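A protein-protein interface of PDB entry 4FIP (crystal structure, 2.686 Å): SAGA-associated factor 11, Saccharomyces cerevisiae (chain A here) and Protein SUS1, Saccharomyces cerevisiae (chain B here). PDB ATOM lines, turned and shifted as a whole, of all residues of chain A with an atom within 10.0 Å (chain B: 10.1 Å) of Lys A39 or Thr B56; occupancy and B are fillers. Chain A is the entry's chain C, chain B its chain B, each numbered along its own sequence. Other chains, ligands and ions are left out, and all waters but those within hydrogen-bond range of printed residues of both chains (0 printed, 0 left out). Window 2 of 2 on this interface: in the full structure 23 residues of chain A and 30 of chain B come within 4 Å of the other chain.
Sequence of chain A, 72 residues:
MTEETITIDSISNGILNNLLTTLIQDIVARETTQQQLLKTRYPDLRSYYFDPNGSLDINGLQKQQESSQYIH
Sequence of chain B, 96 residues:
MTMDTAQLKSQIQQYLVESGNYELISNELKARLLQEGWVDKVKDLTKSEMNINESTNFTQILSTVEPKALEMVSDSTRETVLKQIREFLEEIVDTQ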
ATOM      1  N   VAL A  28     -20.346   4.538 -16.787  1.00  0.00           N
ATOM      2  CA  VAL A  28     -20.625   3.104 -17.072  1.00  0.00           C
ATOM      3  C   VAL A  28     -21.196   2.868 -18.497  1.00  0.00           C
ATOM      4  O   VAL A  28     -20.800   1.898 -19.150  1.00  0.00           O
ATOM      5  CB  VAL A  28     -21.551   2.443 -16.010  1.00  0.00           C
ATOM      6  CG1 VAL A  28     -21.990   1.068 -16.490  1.00  0.00           C
ATOM      7  CG2 VAL A  28     -20.873   2.341 -14.649  1.00  0.00           C
ATOM      8  N   ALA A  29     -22.100   3.741 -18.972  1.00  0.00           N
ATOM      9  CA  ALA A  29     -22.735   3.579 -20.312  1.00  0.00           C
ATOM     10  C   ALA A  29     -21.704   3.704 -21.430  1.00  0.00           C
ATOM     11  O   ALA A  29     -21.727   2.935 -22.385  1.00  0.00           O
ATOM     12  CB  ALA A  29     -23.873   4.580 -20.521  1.00  0.00           C
ATOM     13  N   ARG A  30     -20.781   4.650 -21.286  1.00  0.00           N
ATOM     14  CA  ARG A  30     -19.712   4.821 -22.246  1.00  0.00           C
ATOM     15  C   ARG A  30     -18.745   3.664 -22.225  1.00  0.00           C
ATOM     16  O   ARG A  30     -18.261   3.271 -23.251  1.00  0.00           O
ATOM     17  CB  ARG A  30     -18.940   6.075 -21.938  1.00  0.00           C
ATOM     18  CG  ARG A  30     -19.755   7.362 -22.034  1.00  0.00           C
ATOM     19  CD  ARG A  30     -18.995   8.554 -21.480  1.00  0.00           C
ATOM     20  NE  ARG A  30     -19.831   9.758 -21.414  1.00  0.00           N
ATOM     21  CZ  ARG A  30     -19.843  10.710 -22.341  1.00  0.00           C
ATOM     22  NH1 ARG A  30     -19.086  10.618 -23.420  1.00  0.00           N
ATOM     23  NH2 ARG A  30     -20.612  11.767 -22.195  1.00  0.00           N
ATOM     24  N   GLU A  31     -18.463   3.091 -21.062  1.00  0.00           N
ATOM     25  CA  GLU A  31     -17.596   1.916 -20.996  1.00  0.00           C
ATOM     26  C   GLU A  31     -18.254   0.662 -21.532  1.00  0.00           C
ATOM     27  O   GLU A  31     -17.644  -0.091 -22.324  1.00  0.00           O
ATOM     28  CB  GLU A  31     -17.165   1.649 -19.567  1.00  0.00           C
ATOM     29  CG  GLU A  31     -16.247   2.694 -18.997  1.00  0.00           C
ATOM     30  CD  GLU A  31     -14.935   2.848 -19.768  1.00  0.00           C
ATOM     31  OE1 GLU A  31     -14.580   1.973 -20.634  1.00  0.00           O
ATOM     32  OE2 GLU A  31     -14.232   3.862 -19.491  1.00  0.00           O
ATOM     33  N   THR A  32     -19.489   0.404 -21.102  1.00  0.00           N
ATOM     34  CA  THR A  32     -20.125  -0.858 -21.507  1.00  0.00           C
ATOM     35  C   THR A  32     -20.333  -0.848 -23.005  1.00  0.00           C
ATOM     36  O   THR A  32     -19.959  -1.807 -23.675  1.00  0.00           O
ATOM     37  CB  THR A  32     -21.450  -1.159 -20.806  1.00  0.00           C
ATOM     38  OG1 THR A  32     -22.482  -0.295 -21.310  1.00  0.00           O
ATOM     39  CG2 THR A  32     -21.299  -1.051 -19.301  1.00  0.00           C
ATOM     40  N   THR A  33     -20.881   0.244 -23.545  1.00  0.00           N
ATOM     41  CA  THR A  33     -21.147   0.303 -24.983  1.00  0.00           C
ATOM     42  C   THR A  33     -19.845   0.137 -25.781  1.00  0.00           C
ATOM     43  O   THR A  33     -19.797  -0.504 -26.846  1.00  0.00           O
ATOM     44  CB  THR A  33     -21.847   1.620 -25.385  1.00  0.00           C
ATOM     45  OG1 THR A  33     -21.007   2.730 -25.063  1.00  0.00           O
ATOM     46  CG2 THR A  33     -23.198   1.756 -24.685  1.00  0.00           C
ATOM     47  N   GLN A  34     -18.775   0.709 -25.249  1.00  0.00           N
ATOM     48  CA  GLN A  34     -17.506   0.765 -25.962  1.00  0.00           C
ATOM     49  C   GLN A  34     -16.942  -0.646 -26.111  1.00  0.00           C
ATOM     50  O   GLN A  34     -16.526  -1.049 -27.176  1.00  0.00           O
ATOM     51  CB  GLN A  34     -16.584   1.720 -25.202  1.00  0.00           C
ATOM     52  CG  GLN A  34     -15.201   1.942 -25.751  1.00  0.00           C
ATOM     53  CD  GLN A  34     -14.447   3.011 -24.946  1.00  0.00           C
ATOM     54  OE1 GLN A  34     -15.075   3.839 -24.220  1.00  0.00           O
ATOM     55  NE2 GLN A  34     -13.087   3.011 -25.064  1.00  0.00           N
ATOM     56  N   GLN A  35     -17.005  -1.407 -25.031  1.00  0.00           N
ATOM     57  CA  GLN A  35     -16.449  -2.756 -24.974  1.00  0.00           C
ATOM     58  C   GLN A  35     -17.296  -3.659 -25.834  1.00  0.00           C
ATOM     59  O   GLN A  35     -16.828  -4.630 -26.455  1.00  0.00           O
ATOM     60  CB  GLN A  35     -16.461  -3.209 -23.510  1.00  0.00           C
ATOM     61  CG  GLN A  35     -15.865  -4.550 -23.208  1.00  0.00           C
ATOM     62  CD  GLN A  35     -14.404  -4.690 -23.602  1.00  0.00           C
ATOM     63  OE1 GLN A  35     -13.724  -3.718 -23.857  1.00  0.00           O
ATOM     64  NE2 GLN A  35     -13.922  -5.923 -23.640  1.00  0.00           N
ATOM     65  N   GLN A  36     -18.565  -3.293 -25.888  1.00  0.00           N
ATOM     66  CA  GLN A  36     -19.522  -4.037 -26.641  1.00  0.00           C
ATOM     67  C   GLN A  36     -19.272  -3.795 -28.100  1.00  0.00           C
ATOM     68  O   GLN A  36     -19.345  -4.721 -28.899  1.00  0.00           O
ATOM     69  CB  GLN A  36     -20.907  -3.619 -26.240  1.00  0.00           C
ATOM     70  CG  GLN A  36     -22.024  -4.315 -26.991  1.00  0.00           C
ATOM     71  CD  GLN A  36     -23.335  -3.689 -26.650  1.00  0.00           C
ATOM     72  OE1 GLN A  36     -23.839  -2.852 -27.397  1.00  0.00           O
ATOM     73  NE2 GLN A  36     -23.831  -3.991 -25.449  1.00  0.00           N
ATOM     74  N   LEU A  37     -18.922  -2.586 -28.472  1.00  0.00           N
ATOM     75  CA  LEU A  37     -18.519  -2.380 -29.858  1.00  0.00           C
ATOM     76  C   LEU A  37     -17.248  -3.183 -30.202  1.00  0.00           C
ATOM     77  O   LEU A  37     -17.167  -3.804 -31.265  1.00  0.00           O
ATOM     78  CB  LEU A  37     -18.322  -0.886 -30.133  1.00  0.00           C
ATOM     79  CG  LEU A  37     -17.874  -0.453 -31.523  1.00  0.00           C
ATOM     80  CD1 LEU A  37     -18.756  -1.073 -32.609  1.00  0.00           C
ATOM     81  CD2 LEU A  37     -17.866   1.070 -31.543  1.00  0.00           C
ATOM     82  N   LEU A  38     -16.259  -3.199 -29.308  1.00  0.00           N
ATOM     83  CA  LEU A  38     -15.017  -3.947 -29.583  1.00  0.00           C
ATOM     84  C   LEU A  38     -15.277  -5.444 -29.727  1.00  0.00           C
ATOM     85  O   LEU A  38     -14.771  -6.055 -30.648  1.00  0.00           O
ATOM     86  CB  LEU A  38     -13.883  -3.647 -28.550  1.00  0.00           C
ATOM     87  CG  LEU A  38     -13.227  -2.220 -28.550  1.00  0.00           C
ATOM     88  CD1 LEU A  38     -12.570  -1.933 -27.204  1.00  0.00           C
ATOM     89  CD2 LEU A  38     -12.240  -1.917 -29.676  1.00  0.00           C
ATOM     90  N   LYS A  39     -16.078  -6.036 -28.851  1.00  0.00           N
ATOM     91  CA  LYS A  39     -16.343  -7.479 -28.960  1.00  0.00           C
ATOM     92  C   LYS A  39     -17.176  -7.852 -30.224  1.00  0.00           C
ATOM     93  O   LYS A  39     -17.082  -8.955 -30.733  1.00  0.00           O
ATOM     94  CB  LYS A  39     -17.050  -8.032 -27.713  1.00  0.00           C
ATOM     95  CG  LYS A  39     -16.292  -7.953 -26.393  1.00  0.00           C
ATOM     96  CD  LYS A  39     -17.177  -8.427 -25.217  1.00  0.00           C
ATOM     97  CE  LYS A  39     -16.397  -8.818 -23.938  1.00  0.00           C
ATOM     98  NZ  LYS A  39     -17.197  -9.447 -22.824  1.00  0.00           N
ATOM     99  N   THR A  40     -18.000  -6.955 -30.726  1.00  0.00           N
ATOM    100  CA  THR A  40     -18.783  -7.300 -31.890  1.00  0.00           C
ATOM    101  C   THR A  40     -17.942  -7.159 -33.137  1.00  0.00           C
ATOM    102  O   THR A  40     -17.953  -8.003 -34.002  1.00  0.00           O
ATOM    103  CB  THR A  40     -20.008  -6.391 -31.995  1.00  0.00           C
ATOM    104  OG1 THR A  40     -20.661  -6.321 -30.710  1.00  0.00           O
ATOM    105  CG2 THR A  40     -20.967  -6.895 -33.098  1.00  0.00           C
ATOM    106  N   ARG A  41     -17.217  -6.058 -33.218  1.00  0.00           N
ATOM    107  CA  ARG A  41     -16.369  -5.739 -34.360  1.00  0.00           C
ATOM    108  C   ARG A  41     -15.158  -6.676 -34.529  1.00  0.00           C
ATOM    109  O   ARG A  41     -14.692  -6.903 -35.654  1.00  0.00           O
ATOM    110  CB  ARG A  41     -15.904  -4.291 -34.194  1.00  0.00           C
ATOM    111  CG  ARG A  41     -14.932  -3.816 -35.256  1.00  0.00           C
ATOM    112  CD  ARG A  41     -14.695  -2.330 -35.153  1.00  0.00           C
ATOM    113  NE  ARG A  41     -15.926  -1.561 -35.305  1.00  0.00           N
ATOM    114  CZ  ARG A  41     -15.966  -0.234 -35.375  1.00  0.00           C
ATOM    115  NH1 ARG A  41     -14.870   0.473 -35.314  1.00  0.00           N
ATOM    116  NH2 ARG A  41     -17.110   0.388 -35.520  1.00  0.00           N
ATOM    117  N   TYR A  42     -14.646  -7.207 -33.416  1.00  0.00           N
ATOM    118  CA  TYR A  42     -13.481  -8.092 -33.436  1.00  0.00           C
ATOM    119  C   TYR A  42     -13.649  -9.337 -32.525  1.00  0.00           C
ATOM    120  O   TYR A  42     -13.212  -9.321 -31.363  1.00  0.00           O
ATOM    121  CB  TYR A  42     -12.226  -7.340 -33.000  1.00  0.00           C
ATOM    122  CG  TYR A  42     -12.016  -5.957 -33.570  1.00  0.00           C
ATOM    123  CD1 TYR A  42     -11.671  -5.776 -34.886  1.00  0.00           C
ATOM    124  CD2 TYR A  42     -12.078  -4.829 -32.752  1.00  0.00           C
ATOM    125  CE1 TYR A  42     -11.432  -4.511 -35.398  1.00  0.00           C
ATOM    126  CE2 TYR A  42     -11.832  -3.559 -33.248  1.00  0.00           C
ATOM    127  CZ  TYR A  42     -11.514  -3.402 -34.577  1.00  0.00           C
ATOM    128  OH  TYR A  42     -11.284  -2.133 -35.086  1.00  0.00           O
ATOM    129  N   PRO A  43     -14.269 -10.426 -33.053  1.00  0.00           N
ATOM    130  CA  PRO A  43     -14.387 -11.751 -32.396  1.00  0.00           C
ATOM    131  C   PRO A  43     -13.193 -12.210 -31.544  1.00  0.00           C
ATOM    132  O   PRO A  43     -13.391 -12.702 -30.442  1.00  0.00           O
ATOM    133  CB  PRO A  43     -14.556 -12.693 -33.590  1.00  0.00           C
ATOM    134  CG  PRO A  43     -15.289 -11.862 -34.611  1.00  0.00           C
ATOM    135  CD  PRO A  43     -15.046 -10.407 -34.312  1.00  0.00           C
ATOM    136  N   ASP A  44     -11.978 -12.052 -32.067  1.00  0.00           N
ATOM    137  CA  ASP A  44     -10.753 -12.350 -31.319  1.00  0.00           C
ATOM    138  C   ASP A  44     -10.143 -11.066 -30.743  1.00  0.00           C
ATOM    139  O   ASP A  44     -10.089 -10.046 -31.433  1.00  0.00           O
ATOM    140  CB  ASP A  44      -9.735 -13.060 -32.214  1.00  0.00           C
ATOM    141  CG  ASP A  44      -8.637 -13.770 -31.409  1.00  0.00           C
ATOM    142  OD1 ASP A  44      -8.212 -13.232 -30.359  1.00  0.00           O
ATOM    143  OD2 ASP A  44      -8.188 -14.872 -31.816  1.00  0.00           O
ATOM    144  N   LEU A  45      -9.713 -11.117 -29.477  1.00  0.00           N
ATOM    145  CA  LEU A  45      -8.945 -10.029 -28.840  1.00  0.00           C
ATOM    146  C   LEU A  45      -7.950 -10.569 -27.808  1.00  0.00           C
ATOM    147  O   LEU A  45      -6.752 -10.274 -27.858  1.00  0.00           O
ATOM    148  CB  LEU A  45      -9.866  -9.027 -28.154  1.00  0.00           C
ATOM    149  CG  LEU A  45     -11.226  -8.723 -28.774  1.00  0.00           C
ATOM    150  CD1 LEU A  45     -12.202  -9.859 -28.460  1.00  0.00           C
ATOM    151  CD2 LEU A  45     -11.738  -7.390 -28.241  1.00  0.00           C
ATOM    152  N   THR B  46     -15.320  -0.365 -13.768  1.00  0.00           N
ATOM    153  CA  THR B  46     -16.287  -0.836 -14.731  1.00  0.00           C
ATOM    154  C   THR B  46     -15.617  -1.887 -15.579  1.00  0.00           C
ATOM    155  O   THR B  46     -16.162  -2.942 -15.822  1.00  0.00           O
ATOM    156  CB  THR B  46     -16.809   0.326 -15.599  1.00  0.00           C
ATOM    157  OG1 THR B  46     -17.396   1.297 -14.737  1.00  0.00           O
ATOM    158  CG2 THR B  46     -17.856  -0.134 -16.592  1.00  0.00           C
ATOM    159  N   LYS B  47     -14.416  -1.608 -16.035  1.00  0.00           N
ATOM    160  CA  LYS B  47     -13.753  -2.546 -16.937  1.00  0.00           C
ATOM    161  C   LYS B  47     -13.506  -3.874 -16.201  1.00  0.00           C
ATOM    162  O   LYS B  47     -13.765  -4.946 -16.766  1.00  0.00           O
ATOM    163  CB  LYS B  47     -12.444  -1.953 -17.523  1.00  0.00           C
ATOM    164  CG  LYS B  47     -12.644  -0.805 -18.507  1.00  0.00           C
ATOM    165  CD  LYS B  47     -11.408  -0.608 -19.387  1.00  0.00           C
ATOM    166  CE  LYS B  47     -11.377   0.765 -20.089  1.00  0.00           C
ATOM    167  NZ  LYS B  47     -11.105   1.964 -19.205  1.00  0.00           N
ATOM    168  N   SER B  48     -13.051  -3.789 -14.947  1.00  0.00           N
ATOM    169  CA  SER B  48     -12.820  -4.966 -14.076  1.00  0.00           C
ATOM    170  C   SER B  48     -14.063  -5.814 -13.809  1.00  0.00           C
ATOM    171  O   SER B  48     -13.967  -7.031 -13.778  1.00  0.00           O
ATOM    172  CB  SER B  48     -12.255  -4.517 -12.723  1.00  0.00           C
ATOM    173  OG  SER B  48     -12.341  -5.565 -11.757  1.00  0.00           O
ATOM    174  N   GLU B  49     -15.212  -5.167 -13.572  1.00  0.00           N
ATOM    175  CA  GLU B  49     -16.471  -5.895 -13.398  1.00  0.00           C
ATOM    176  C   GLU B  49     -16.938  -6.513 -14.702  1.00  0.00           C
ATOM    177  O   GLU B  49     -17.537  -7.574 -14.680  1.00  0.00           O
ATOM    178  CB  GLU B  49     -17.583  -5.025 -12.823  1.00  0.00           C
ATOM    179  CG  GLU B  49     -17.276  -4.421 -11.452  1.00  0.00           C
ATOM    180  CD  GLU B  49     -17.151  -5.416 -10.290  1.00  0.00           C
ATOM    181  OE1 GLU B  49     -18.019  -6.302 -10.135  1.00  0.00           O
ATOM    182  OE2 GLU B  49     -16.189  -5.272  -9.494  1.00  0.00           O
ATOM    183  N   MET B  50     -16.652  -5.878 -15.837  1.00  0.00           N
ATOM    184  CA  MET B  50     -16.970  -6.492 -17.132  1.00  0.00           C
ATOM    185  C   MET B  50     -16.192  -7.772 -17.310  1.00  0.00           C
ATOM    186  O   MET B  50     -16.674  -8.733 -17.912  1.00  0.00           O
ATOM    187  CB  MET B  50     -16.703  -5.555 -18.315  1.00  0.00           C
ATOM    188  CG  MET B  50     -17.819  -4.537 -18.578  1.00  0.00           C
ATOM    189  SD  MET B  50     -17.691  -3.558 -20.106  1.00  0.00           S
ATOM    190  CE  MET B  50     -16.523  -2.311 -19.579  1.00  0.00           C
ATOM    191  N   ASN B  51     -14.986  -7.789 -16.774  1.00  0.00           N
ATOM    192  CA  ASN B  51     -14.129  -8.945 -16.931  1.00  0.00           C
ATOM    193  C   ASN B  51     -14.544 -10.033 -15.990  1.00  0.00           C
ATOM    194  O   ASN B  51     -14.742 -11.169 -16.400  1.00  0.00           O
ATOM    195  CB  ASN B  51     -12.684  -8.587 -16.641  1.00  0.00           C
ATOM    196  CG  ASN B  51     -11.796  -8.931 -17.778  1.00  0.00           C
ATOM    197  OD1 ASN B  51     -11.491  -8.058 -18.591  1.00  0.00           O
ATOM    198  ND2 ASN B  51     -11.433 -10.211 -17.902  1.00  0.00           N
ATOM    199  N   ILE B  52     -14.649  -9.664 -14.717  1.00  0.00           N
ATOM    200  CA  ILE B  52     -15.029 -10.567 -13.645  1.00  0.00           C
ATOM    201  C   ILE B  52     -16.355 -11.250 -13.933  1.00  0.00           C
ATOM    202  O   ILE B  52     -16.507 -12.428 -13.632  1.00  0.00           O
ATOM    203  CB  ILE B  52     -15.163  -9.802 -12.320  1.00  0.00           C
ATOM    204  CG1 ILE B  52     -13.788  -9.445 -11.738  1.00  0.00           C
ATOM    205  CG2 ILE B  52     -15.993 -10.599 -11.340  1.00  0.00           C
ATOM    206  CD1 ILE B  52     -13.824  -8.271 -10.777  1.00  0.00           C
ATOM    207  N   ASN B  53     -17.306 -10.516 -14.526  1.00  0.00           N
ATOM    208  CA  ASN B  53     -18.647 -11.051 -14.840  1.00  0.00           C
ATOM    209  C   ASN B  53     -18.858 -11.489 -16.297  1.00  0.00           C
ATOM    210  O   ASN B  53     -19.927 -11.965 -16.635  1.00  0.00           O
ATOM    211  CB  ASN B  53     -19.729 -10.052 -14.415  1.00  0.00           C
ATOM    212  CG  ASN B  53     -19.680  -9.743 -12.917  1.00  0.00           C
ATOM    213  OD1 ASN B  53     -20.131 -10.526 -12.105  1.00  0.00           O
ATOM    214  ND2 ASN B  53     -19.130  -8.606 -12.558  1.00  0.00           N
ATOM    215  N   GLU B  54     -17.833 -11.363 -17.142  1.00  0.00           N
ATOM    216  CA  GLU B  54     -17.921 -11.783 -18.544  1.00  0.00           C
ATOM    217  C   GLU B  54     -19.141 -11.174 -19.253  1.00  0.00           C
ATOM    218  O   GLU B  54     -19.801 -11.828 -20.064  1.00  0.00           O
ATOM    219  CB  GLU B  54     -18.003 -13.309 -18.630  1.00  0.00           C
ATOM    220  CG  GLU B  54     -16.786 -14.054 -18.117  1.00  0.00           C
ATOM    221  CD  GLU B  54     -15.655 -14.058 -19.121  1.00  0.00           C
ATOM    222  OE1 GLU B  54     -15.740 -14.877 -20.073  1.00  0.00           O
ATOM    223  OE2 GLU B  54     -14.691 -13.261 -18.944  1.00  0.00           O
ATOM    224  N   SER B  55     -19.442  -9.921 -18.945  1.00  0.00           N
ATOM    225  CA  SER B  55     -20.627  -9.294 -19.458  1.00  0.00           C
ATOM    226  C   SER B  55     -20.343  -7.865 -19.828  1.00  0.00           C
ATOM    227  O   SER B  55     -19.457  -7.254 -19.270  1.00  0.00           O
ATOM    228  CB  SER B  55     -21.732  -9.361 -18.395  1.00  0.00           C
ATOM    229  OG  SER B  55     -22.983  -8.844 -18.855  1.00  0.00           O
ATOM    230  N   THR B  56     -21.105  -7.350 -20.788  1.00  0.00           N
ATOM    231  CA  THR B  56     -21.147  -5.911 -21.139  1.00  0.00           C
ATOM    232  C   THR B  56     -22.551  -5.315 -20.983  1.00  0.00           C
ATOM    233  O   THR B  56     -22.796  -4.175 -21.378  1.00  0.00           O
ATOM    234  CB  THR B  56     -20.701  -5.674 -22.606  1.00  0.00           C
ATOM    235  OG1 THR B  56     -21.562  -6.397 -23.499  1.00  0.00           O
ATOM    236  CG2 THR B  56     -19.290  -6.126 -22.825  1.00  0.00           C
ATOM    237  N   ASN B  57     -23.483  -6.092 -20.436  1.00  0.00           N
ATOM    238  CA  ASN B  57     -24.863  -5.653 -20.241  1.00  0.00           C
ATOM    239  C   ASN B  57     -24.912  -4.549 -19.190  1.00  0.00           C
ATOM    240  O   ASN B  57     -24.552  -4.773 -18.023  1.00  0.00           O
ATOM    241  CB  ASN B  57     -25.692  -6.835 -19.785  1.00  0.00           C
ATOM    242  CG  ASN B  57     -27.121  -6.476 -19.485  1.00  0.00           C
ATOM    243  OD1 ASN B  57     -27.985  -6.793 -20.273  1.00  0.00           O
ATOM    244  ND2 ASN B  57     -27.382  -5.834 -18.348  1.00  0.00           N
ATOM    245  N   PHE B  58     -25.358  -3.360 -19.606  1.00  0.00           N
ATOM    246  CA  PHE B  58     -25.382  -2.179 -18.732  1.00  0.00           C
ATOM    247  C   PHE B  58     -25.989  -2.427 -17.335  1.00  0.00           C
ATOM    248  O   PHE B  58     -25.361  -2.157 -16.322  1.00  0.00           O
ATOM    249  CB  PHE B  58     -26.109  -1.022 -19.418  1.00  0.00           C
ATOM    250  CG  PHE B  58     -26.169   0.222 -18.571  1.00  0.00           C
ATOM    251  CD1 PHE B  58     -25.050   0.997 -18.394  1.00  0.00           C
ATOM    252  CD2 PHE B  58     -27.334   0.574 -17.908  1.00  0.00           C
ATOM    253  CE1 PHE B  58     -25.079   2.105 -17.584  1.00  0.00           C
ATOM    254  CE2 PHE B  58     -27.373   1.687 -17.082  1.00  0.00           C
ATOM    255  CZ  PHE B  58     -26.236   2.452 -16.922  1.00  0.00           C
ATOM    256  N   THR B  59     -27.210  -2.937 -17.293  1.00  0.00           N
ATOM    257  CA  THR B  59     -27.945  -3.051 -16.038  1.00  0.00           C
ATOM    258  C   THR B  59     -27.226  -3.908 -15.013  1.00  0.00           C
ATOM    259  O   THR B  59     -27.132  -3.569 -13.829  1.00  0.00           O
ATOM    260  CB  THR B  59     -29.308  -3.676 -16.293  1.00  0.00           C
ATOM    261  OG1 THR B  59     -29.958  -2.906 -17.292  1.00  0.00           O
ATOM    262  CG2 THR B  59     -30.153  -3.663 -15.034  1.00  0.00           C
ATOM    263  N   GLN B  60     -26.758  -5.044 -15.490  1.00  0.00           N
ATOM    264  CA  GLN B  60     -26.035  -5.989 -14.674  1.00  0.00           C
ATOM    265  C   GLN B  60     -24.768  -5.363 -14.105  1.00  0.00           C
ATOM    266  O   GLN B  60     -24.497  -5.465 -12.909  1.00  0.00           O
ATOM    267  CB  GLN B  60     -25.708  -7.225 -15.521  1.00  0.00           C
ATOM    268  CG  GLN B  60     -24.699  -8.159 -14.878  1.00  0.00           C
ATOM    269  CD  GLN B  60     -24.644  -9.542 -15.496  1.00  0.00           C
ATOM    270  OE1 GLN B  60     -25.373  -9.860 -16.455  1.00  0.00           O
ATOM    271  NE2 GLN B  60     -23.780 -10.388 -14.934  1.00  0.00           N
ATOM    272  N   ILE B  61     -23.996  -4.708 -14.968  1.00  0.00           N
ATOM    273  CA  ILE B  61     -22.707  -4.134 -14.567  1.00  0.00           C
ATOM    274  C   ILE B  61     -22.921  -2.952 -13.636  1.00  0.00           C
ATOM    275  O   ILE B  61     -22.236  -2.834 -12.608  1.00  0.00           O
ATOM    276  CB  ILE B  61     -21.837  -3.758 -15.800  1.00  0.00           C
ATOM    277  CG1 ILE B  61     -21.314  -5.044 -16.470  1.00  0.00           C
ATOM    278  CG2 ILE B  61     -20.640  -2.891 -15.421  1.00  0.00           C
ATOM    279  CD1 ILE B  61     -20.375  -5.919 -15.637  1.00  0.00           C
ATOM    280  N   LEU B  62     -23.896  -2.105 -13.985  1.00  0.00           N
ATOM    281  CA  LEU B  62     -24.294  -0.969 -13.147  1.00  0.00           C
ATOM    282  C   LEU B  62     -24.516  -1.377 -11.717  1.00  0.00           C
ATOM    283  O   LEU B  62     -24.063  -0.703 -10.825  1.00  0.00           O
ATOM    284  CB  LEU B  62     -25.568  -0.329 -13.659  1.00  0.00           C
ATOM    285  CG  LEU B  62     -25.960   0.976 -12.936  1.00  0.00           C
ATOM    286  CD1 LEU B  62     -24.824   2.015 -12.927  1.00  0.00           C
ATOM    287  CD2 LEU B  62     -27.245   1.498 -13.568  1.00  0.00           C
ATOM    288  N   THR B  64     -23.371  -3.672  -9.838  1.00  0.00           N
ATOM    289  CA  THR B  64     -22.175  -3.992  -9.059  1.00  0.00           C
ATOM    290  C   THR B  64     -21.223  -2.782  -8.977  1.00  0.00           C
ATOM    291  O   THR B  64     -20.432  -2.674  -8.030  1.00  0.00           O
ATOM    292  CB  THR B  64     -21.423  -5.192  -9.681  1.00  0.00           C
ATOM    293  OG1 THR B  64     -21.318  -5.005 -11.106  1.00  0.00           O
ATOM    294  CG2 THR B  64     -22.167  -6.512  -9.382  1.00  0.00           C
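Thr B46 touches Val A28.
CG1 of Val A28 touches CE1 of Phe B58, 3.4 Å away.
N of Ala A29 touches CE1 of Phe B58, at 3.7 Å.
Glu A31 touches Thr B46 (CB to CG2, 3.5 Å).
Met B50 touches Glu A31 (CE to O, 3.7 Å).
Thr A32 touches Met B50.
Thr A32 touches Thr B56.
Gln A35 touches Thr B56.
Gln A36 touches Thr B56 (NE2 to OG1, 3.8 Å).
NZ of Lys A39 touches CG2 of Thr B56, at 3.9 Å.
O of Met B50 sits at hydrogen-bond distance from N of Ser B55.
O of Ala A29 lies within hydrogen-bond range of OG1 of Thr A33, 2.8 Å away.
The backbone carbonyl oxygen of Ala A29 lies within hydrogen-bond range of the side-chain hydroxyl of Thr A32, at 3.5 Å.
The backbone carbonyl oxygen of Gln A36 sits at hydrogen-bond distance from the side-chain hydroxyl of Thr A40 (2.8 Å).
Of the 18 printed residues of chain A, 7 touch a printed residue of chain B.
Printed residues of chain B that touch a printed residue of chain A: Thr B46, Lys B47, Met B50, Thr B56 and Phe B58.
Hydrophobic or aromatic side chains of chain B within 4 Å of the printed part of chain A: Met B50 and Phe B58.
Among the printed residues, Asp or Glu carboxylates within 4 Å of a Lys or Arg side-chain nitrogen of the other chain: Glu A31 with Lys B47.
The side-chain amino group of Lys B47 is in salt-bridge range of the side-chain carboxylate of Glu A31, at 3.7 Å.
Printed residues of chain B within 4 Å of Val A28: Thr B46 (3.6 Å) and Phe B58 (3.4 Å).
Of the printed residues of chain B, Ala A29 touches Phe B58 (3.7 Å).
Of the printed residues of chain B, Glu A31 touches Thr B46 (3.5 Å), Lys B47 (3.5 Å) and Met B50 (3.7 Å).
Thr A32 touches just these residues of chain B: Met B50 and Thr B56.
Gln A34 touches none of the printed residues of chain B.
No residue of chain B comes within 4 Å of Leu A38.
Of chain B, only Thr B56 (3.9 Å) comes within 4 Å of Lys A39.
No residue of chain B comes within 4 Å of Thr A40.
Of the printed residues of chain A, Thr B46 touches Val A28 and Glu A31.
Printed residues of chain A within 4 Å of Lys B47: Glu A31.
No residue of chain A comes within 4 Å of Ser B55.
Thr B56 touches just these residues of chain A: Thr A32 (3.4 Å), Gln A35 (3.8 Å), Gln A36 (3.8 Å) and Lys A39 (3.9 Å).
No residue of chain A comes within 4 Å of Asn B57.
The nearest residue of chain B that does not touch Lys A39 is Glu B54 (4.4 Å).
The nearest printed residue of chain A that does not touch Phe B58 is Thr A32 (4.1 Å).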
